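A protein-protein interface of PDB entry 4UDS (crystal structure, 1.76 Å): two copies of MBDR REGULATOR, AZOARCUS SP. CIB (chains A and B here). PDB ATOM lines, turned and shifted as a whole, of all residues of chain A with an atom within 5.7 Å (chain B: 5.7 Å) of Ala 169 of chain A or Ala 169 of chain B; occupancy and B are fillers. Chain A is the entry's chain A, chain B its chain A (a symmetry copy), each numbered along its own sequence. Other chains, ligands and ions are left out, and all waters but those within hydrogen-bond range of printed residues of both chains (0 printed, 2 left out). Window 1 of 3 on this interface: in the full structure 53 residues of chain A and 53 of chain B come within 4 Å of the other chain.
Printed residues of chain B within 4 Å of Ala 169 of chain A: Ala 169, Ala 170, Gly 173 and Val 174. Ala 169 of chain B touches just these residues of chain A: Ala 169, Ala 170, Gly 173 and Val 174. Of the printed residues of chain A, Ile 166 of chain B touches Val 174 (3.8 Å). Printed residues of chain A within 4 Å of Val 174 of chain B: Ile 166 (3.8 Å) and Ala 169 (3.5 Å). Of the printed residues of chain A, Ala 170 of chain B touches Ala 169 (3.8 Å). Of the printed residues of chain B, Gly 173 of chain A touches Ala 169. Tyr 134 of chain A touches none of the printed residues of chain B. Asp 172 of chain B touches none of the printed residues of chain A. The nearest printed residue of chain B that does not touch Ile 166 of chain A is Ala 170 of chain B (4.9 Å).
Ile 166 of chain A touches Val 174 of chain B, and with the chains exchanged Val 174 of chain A touches Ile 166 of chain B. Ala 169 of chain A touches its own counterpart, Ala 169 of chain B. Ala 169 of chain A touches Ala 170 of chain B, and with the chains exchanged Ala 170 of chain A touches Ala 169 of chain B. Ala 169 of chain A touches Gly 173 of chain B, and with the chains exchanged Gly 173 of chain A touches Ala 169 of chain B. Of the 9 pairs that touch across the chains among the printed residues, 9 have their exchanged pair printed and touching as well.
Of the 12 printed residues of chain B, 5 touch a printed residue of chain A. Hydrophobic or aromatic side chains of chain B within 4 Å of the printed part of chain A: Ile 166, Ala 169 and Val 174. Hydrophobic or aromatic side chains of chain A within 4 Å of the printed part of chain B: Ile 166, Ala 169 and Val 174. Among the printed residues, 9 pairs touch across the chains. Among the printed residues, no Asp or Glu carboxylate lies within 4 Å of a Lys or Arg side-chain nitrogen of the other chain.
CD1 of Ile 166 of chain A touches CG2 of Val 174 of chain B, at 3.8 Å. Ala 169 of chain A touches Ala 170 of chain B. CB of Ala 169 of chain A touches C of Gly 173 of chain B (3.5 Å). CB of Ala 169 of chain A touches N of Val 174 of chain B, at 3.5 Å. O of Ala 170 of chain A touches CB of Ala 169 of chain B (3.8 Å). Gly 173 of chain A touches Ala 169 of chain B. Ile 166 of chain B touches Val 174 of chain A (CD1 to CG2, 3.8 Å). N of Val 174 of chain A touches CB of Ala 169 of chain B, at 3.5 Å.
O of Ala 169 of chain B sits close to O of Ala 169 of chain A (3.4 Å).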
ATOM      1  N   TYR A 134      -6.622  -6.633  25.326  1.00  0.00           N
ATOM      2  CA  TYR A 134      -5.752  -7.786  25.515  1.00  0.00           C
ATOM      3  C   TYR A 134      -6.458  -9.045  25.126  1.00  0.00           C
ATOM      4  O   TYR A 134      -5.929  -9.849  24.405  1.00  0.00           O
ATOM      5  CB  TYR A 134      -5.275  -7.895  26.989  1.00  0.00           C
ATOM      6  CG  TYR A 134      -4.092  -8.833  27.185  1.00  0.00           C
ATOM      7  CD1 TYR A 134      -4.279 -10.156  27.385  1.00  0.00           C
ATOM      8  CD2 TYR A 134      -2.797  -8.362  27.147  1.00  0.00           C
ATOM      9  CE1 TYR A 134      -3.207 -11.017  27.540  1.00  0.00           C
ATOM     10  CE2 TYR A 134      -1.721  -9.206  27.317  1.00  0.00           C
ATOM     11  CZ  TYR A 134      -1.947 -10.538  27.530  1.00  0.00           C
ATOM     12  OH  TYR A 134      -0.923 -11.402  27.672  1.00  0.00           O
ATOM     13  N   ALA A 164      -2.135 -20.878  24.333  1.00  0.00           N
ATOM     14  CA  ALA A 164      -2.163 -19.496  23.875  1.00  0.00           C
ATOM     15  C   ALA A 164      -1.686 -18.543  24.987  1.00  0.00           C
ATOM     16  O   ALA A 164      -1.029 -17.604  24.753  1.00  0.00           O
ATOM     17  CB  ALA A 164      -3.546 -19.099  23.399  1.00  0.00           C
ATOM     18  N   SER A 165      -2.088 -18.847  26.206  1.00  0.00           N
ATOM     19  CA  SER A 165      -1.647 -18.041  27.318  1.00  0.00           C
ATOM     20  C   SER A 165      -0.131 -18.091  27.451  1.00  0.00           C
ATOM     21  O   SER A 165       0.461 -17.146  27.853  1.00  0.00           O
ATOM     22  CB  SER A 165      -2.292 -18.498  28.587  1.00  0.00           C
ATOM     23  OG  SER A 165      -3.627 -18.149  28.560  1.00  0.00           O
ATOM     24  N   ILE A 166       0.443 -19.248  27.195  1.00  0.00           N
ATOM     25  CA  ILE A 166       1.882 -19.370  27.254  1.00  0.00           C
ATOM     26  C   ILE A 166       2.568 -18.539  26.168  1.00  0.00           C
ATOM     27  O   ILE A 166       3.534 -17.930  26.415  1.00  0.00           O
ATOM     28  CB  ILE A 166       2.407 -20.806  27.210  1.00  0.00           C
ATOM     29  CG1 ILE A 166       1.805 -21.652  28.328  1.00  0.00           C
ATOM     30  CG2 ILE A 166       3.895 -20.774  27.409  1.00  0.00           C
ATOM     31  CD1 ILE A 166       1.812 -20.991  29.679  1.00  0.00           C
ATOM     32  N   VAL A 167       2.025 -18.568  24.973  1.00  0.00           N
ATOM     33  CA  VAL A 167       2.576 -17.738  23.938  1.00  0.00           C
ATOM     34  C   VAL A 167       2.473 -16.245  24.293  1.00  0.00           C
ATOM     35  O   VAL A 167       3.416 -15.550  24.152  1.00  0.00           O
ATOM     36  CB  VAL A 167       1.853 -18.000  22.598  1.00  0.00           C
ATOM     37  CG1 VAL A 167       2.295 -17.012  21.518  1.00  0.00           C
ATOM     38  CG2 VAL A 167       2.091 -19.437  22.147  1.00  0.00           C
ATOM     39  N   MET A 168       1.315 -15.804  24.748  1.00  0.00           N
ATOM     40  CA  MET A 168       1.189 -14.421  25.171  1.00  0.00           C
ATOM     41  C   MET A 168       2.070 -14.112  26.351  1.00  0.00           C
ATOM     42  O   MET A 168       2.633 -13.069  26.381  1.00  0.00           O
ATOM     43  CB  MET A 168      -0.267 -14.059  25.492  1.00  0.00           C
ATOM     44  CG  MET A 168      -1.207 -14.274  24.345  1.00  0.00           C
ATOM     45  SD  MET A 168      -0.973 -12.759  23.078  1.00  0.00           S
ATOM     46  CE  MET A 168      -1.493 -11.274  24.306  1.00  0.00           C
ATOM     47  N   ALA A 169       2.186 -15.002  27.324  1.00  0.00           N
ATOM     48  CA  ALA A 169       3.030 -14.730  28.484  1.00  0.00           C
ATOM     49  C   ALA A 169       4.495 -14.521  28.135  1.00  0.00           C
ATOM     50  O   ALA A 169       5.104 -13.664  28.634  1.00  0.00           O
ATOM     51  CB  ALA A 169       2.946 -15.872  29.471  1.00  0.00           C
ATOM     52  N   ALA A 170       5.022 -15.388  27.253  1.00  0.00           N
ATOM     53  CA  ALA A 170       6.395 -15.253  26.809  1.00  0.00           C
ATOM     54  C   ALA A 170       6.585 -13.940  26.101  1.00  0.00           C
ATOM     55  O   ALA A 170       7.554 -13.293  26.282  1.00  0.00           O
ATOM     56  CB  ALA A 170       6.804 -16.383  25.869  1.00  0.00           C
ATOM     57  N   HIS A 171       5.620 -13.598  25.291  1.00  0.00           N
ATOM     58  CA  HIS A 171       5.713 -12.343  24.601  1.00  0.00           C
ATOM     59  C   HIS A 171       5.721 -11.152  25.538  1.00  0.00           C
ATOM     60  O   HIS A 171       6.525 -10.294  25.391  1.00  0.00           O
ATOM     61  CB  HIS A 171       4.621 -12.175  23.578  1.00  0.00           C
ATOM     62  CG  HIS A 171       4.957 -12.846  22.292  1.00  0.00           C
ATOM     63  ND1 HIS A 171       4.717 -14.171  22.088  1.00  0.00           N
ATOM     64  CD2 HIS A 171       5.656 -12.424  21.213  1.00  0.00           C
ATOM     65  CE1 HIS A 171       5.149 -14.524  20.898  1.00  0.00           C
ATOM     66  NE2 HIS A 171       5.741 -13.485  20.350  1.00  0.00           N
ATOM     67  N   ASP A 172       4.832 -11.139  26.510  1.00  0.00           N
ATOM     68  CA  ASP A 172       4.803 -10.045  27.449  1.00  0.00           C
ATOM     69  C   ASP A 172       6.140  -9.934  28.214  1.00  0.00           C
ATOM     70  O   ASP A 172       6.647  -8.918  28.374  1.00  0.00           O
ATOM     71  CB  ASP A 172       3.709 -10.286  28.483  1.00  0.00           C
ATOM     72  CG  ASP A 172       2.291 -10.383  27.879  1.00  0.00           C
ATOM     73  OD1 ASP A 172       2.033 -10.143  26.720  1.00  0.00           O
ATOM     74  OD2 ASP A 172       1.424 -10.624  28.642  1.00  0.00           O
ATOM     75  N   GLY A 173       6.656 -11.044  28.678  1.00  0.00           N
ATOM     76  CA  GLY A 173       7.873 -11.066  29.463  1.00  0.00           C
ATOM     77  C   GLY A 173       9.093 -10.594  28.721  1.00  0.00           C
ATOM     78  O   GLY A 173       9.960 -10.002  29.263  1.00  0.00           O
ATOM     79  N   VAL A 174       9.162 -10.923  27.451  1.00  0.00           N
ATOM     80  CA  VAL A 174      10.293 -10.539  26.644  1.00  0.00           C
ATOM     81  C   VAL A 174      10.325  -9.022  26.523  1.00  0.00           C
ATOM     82  O   VAL A 174      11.351  -8.448  26.511  1.00  0.00           O
ATOM     83  CB  VAL A 174      10.257 -11.264  25.280  1.00  0.00           C
ATOM     84  CG1 VAL A 174      11.009 -10.573  24.234  1.00  0.00           C
ATOM     85  CG2 VAL A 174      10.780 -12.654  25.413  1.00  0.00           C
ATOM     86  N   TYR B 134      16.432  -9.636  40.690  1.00  0.00           N
ATOM     87  CA  TYR B 134      16.002 -10.326  39.481  1.00  0.00           C
ATOM     88  C   TYR B 134      17.165 -10.981  38.809  1.00  0.00           C
ATOM     89  O   TYR B 134      17.101 -12.128  38.451  1.00  0.00           O
ATOM     90  CB  TYR B 134      15.317  -9.346  38.488  1.00  0.00           C
ATOM     91  CG  TYR B 134      14.524 -10.039  37.389  1.00  0.00           C
ATOM     92  CD1 TYR B 134      15.119 -10.429  36.241  1.00  0.00           C
ATOM     93  CD2 TYR B 134      13.179 -10.304  37.542  1.00  0.00           C
ATOM     94  CE1 TYR B 134      14.408 -11.080  35.249  1.00  0.00           C
ATOM     95  CE2 TYR B 134      12.455 -10.936  36.555  1.00  0.00           C
ATOM     96  CZ  TYR B 134      13.088 -11.306  35.399  1.00  0.00           C
ATOM     97  OH  TYR B 134      12.424 -11.953  34.422  1.00  0.00           O
ATOM     98  N   ALA B 164      17.499 -18.665  28.800  1.00  0.00           N
ATOM     99  CA  ALA B 164      17.130 -18.382  30.179  1.00  0.00           C
ATOM    100  C   ALA B 164      16.144 -17.201  30.248  1.00  0.00           C
ATOM    101  O   ALA B 164      15.258 -17.182  31.012  1.00  0.00           O
ATOM    102  CB  ALA B 164      18.351 -18.099  31.031  1.00  0.00           C
ATOM    103  N   SER B 165      16.382 -16.212  29.409  1.00  0.00           N
ATOM    104  CA  SER B 165      15.481 -15.087  29.365  1.00  0.00           C
ATOM    105  C   SER B 165      14.083 -15.533  28.958  1.00  0.00           C
ATOM    106  O   SER B 165      13.131 -14.973  29.389  1.00  0.00           O
ATOM    107  CB  SER B 165      15.985 -14.044  28.421  1.00  0.00           C
ATOM    108  OG  SER B 165      17.092 -13.436  28.978  1.00  0.00           O
ATOM    109  N   ILE B 166      14.012 -16.482  28.048  1.00  0.00           N
ATOM    110  CA  ILE B 166      12.724 -16.995  27.638  1.00  0.00           C
ATOM    111  C   ILE B 166      12.015 -17.729  28.777  1.00  0.00           C
ATOM    112  O   ILE B 166      10.869 -17.582  28.948  1.00  0.00           O
ATOM    113  CB  ILE B 166      12.754 -17.885  26.394  1.00  0.00           C
ATOM    114  CG1 ILE B 166      13.385 -17.161  25.208  1.00  0.00           C
ATOM    115  CG2 ILE B 166      11.341 -18.229  26.022  1.00  0.00           C
ATOM    116  CD1 ILE B 166      12.886 -15.758  25.000  1.00  0.00           C
ATOM    117  N   VAL B 167      12.754 -18.522  29.517  1.00  0.00           N
ATOM    118  CA  VAL B 167      12.159 -19.168  30.653  1.00  0.00           C
ATOM    119  C   VAL B 167      11.662 -18.147  31.690  1.00  0.00           C
ATOM    120  O   VAL B 167      10.582 -18.267  32.150  1.00  0.00           O
ATOM    121  CB  VAL B 167      13.174 -20.126  31.319  1.00  0.00           C
ATOM    122  CG1 VAL B 167      12.631 -20.696  32.630  1.00  0.00           C
ATOM    123  CG2 VAL B 167      13.545 -21.247  30.355  1.00  0.00           C
ATOM    124  N   MET B 168      12.481 -17.166  32.023  1.00  0.00           N
ATOM    125  CA  MET B 168      12.030 -16.132  32.937  1.00  0.00           C
ATOM    126  C   MET B 168      10.886 -15.339  32.368  1.00  0.00           C
ATOM    127  O   MET B 168       9.999 -15.025  33.089  1.00  0.00           O
ATOM    128  CB  MET B 168      13.175 -15.193  33.336  1.00  0.00           C
ATOM    129  CG  MET B 168      14.334 -15.896  33.976  1.00  0.00           C
ATOM    130  SD  MET B 168      13.835 -16.299  35.858  1.00  0.00           S
ATOM    131  CE  MET B 168      13.554 -14.427  36.489  1.00  0.00           C
ATOM    132  N   ALA B 169      10.903 -15.005  31.087  1.00  0.00           N
ATOM    133  CA  ALA B 169       9.809 -14.231  30.506  1.00  0.00           C
ATOM    134  C   ALA B 169       8.461 -14.930  30.584  1.00  0.00           C
ATOM    135  O   ALA B 169       7.506 -14.338  30.887  1.00  0.00           O
ATOM    136  CB  ALA B 169      10.094 -13.934  29.052  1.00  0.00           C
ATOM    137  N   ALA B 170       8.453 -16.236  30.263  1.00  0.00           N
ATOM    138  CA  ALA B 170       7.233 -17.014  30.351  1.00  0.00           C
ATOM    139  C   ALA B 170       6.736 -17.042  31.770  1.00  0.00           C
ATOM    140  O   ALA B 170       5.587 -16.932  32.008  1.00  0.00           O
ATOM    141  CB  ALA B 170       7.435 -18.448  29.872  1.00  0.00           C
ATOM    142  N   HIS B 171       7.658 -17.202  32.681  1.00  0.00           N
ATOM    143  CA  HIS B 171       7.267 -17.209  34.062  1.00  0.00           C
ATOM    144  C   HIS B 171       6.661 -15.895  34.511  1.00  0.00           C
ATOM    145  O   HIS B 171       5.653 -15.895  35.133  1.00  0.00           O
ATOM    146  CB  HIS B 171       8.407 -17.579  34.973  1.00  0.00           C
ATOM    147  CG  HIS B 171       8.583 -19.054  35.071  1.00  0.00           C
ATOM    148  ND1 HIS B 171       9.307 -19.755  34.154  1.00  0.00           N
ATOM    149  CD2 HIS B 171       8.004 -19.978  35.872  1.00  0.00           C
ATOM    150  CE1 HIS B 171       9.265 -21.037  34.439  1.00  0.00           C
ATOM    151  NE2 HIS B 171       8.465 -21.204  35.469  1.00  0.00           N
ATOM    152  N   ASP B 172       7.283 -14.788  34.159  1.00  0.00           N
ATOM    153  CA  ASP B 172       6.745 -13.505  34.536  1.00  0.00           C
ATOM    154  C   ASP B 172       5.332 -13.299  33.946  1.00  0.00           C
ATOM    155  O   ASP B 172       4.481 -12.873  34.585  1.00  0.00           O
ATOM    156  CB  ASP B 172       7.631 -12.395  33.983  1.00  0.00           C
ATOM    157  CG  ASP B 172       9.082 -12.434  34.512  1.00  0.00           C
ATOM    158  OD1 ASP B 172       9.459 -13.172  35.395  1.00  0.00           O
ATOM    159  OD2 ASP B 172       9.813 -11.624  34.064  1.00  0.00           O
ATOM    160  N   GLY B 173       5.159 -13.622  32.689  1.00  0.00           N
ATOM    161  CA  GLY B 173       3.899 -13.421  32.004  1.00  0.00           C
ATOM    162  C   GLY B 173       2.759 -14.230  32.559  1.00  0.00           C
ATOM    163  O   GLY B 173       1.652 -13.817  32.573  1.00  0.00           O
ATOM    164  N   VAL B 174       3.057 -15.439  32.977  1.00  0.00           N
ATOM    165  CA  VAL B 174       2.042 -16.311  33.514  1.00  0.00           C
ATOM    166  C   VAL B 174       1.505 -15.712  34.807  1.00  0.00           C
ATOM    167  O   VAL B 174       0.366 -15.813  35.081  1.00  0.00           O
ATOM    168  CB  VAL B 174       2.594 -17.745  33.683  1.00  0.00           C
ATOM    169  CG1 VAL B 174       1.865 -18.535  34.675  1.00  0.00           C
ATOM    170  CG2 VAL B 174       2.574 -18.469  32.380  1.00  0.00           C
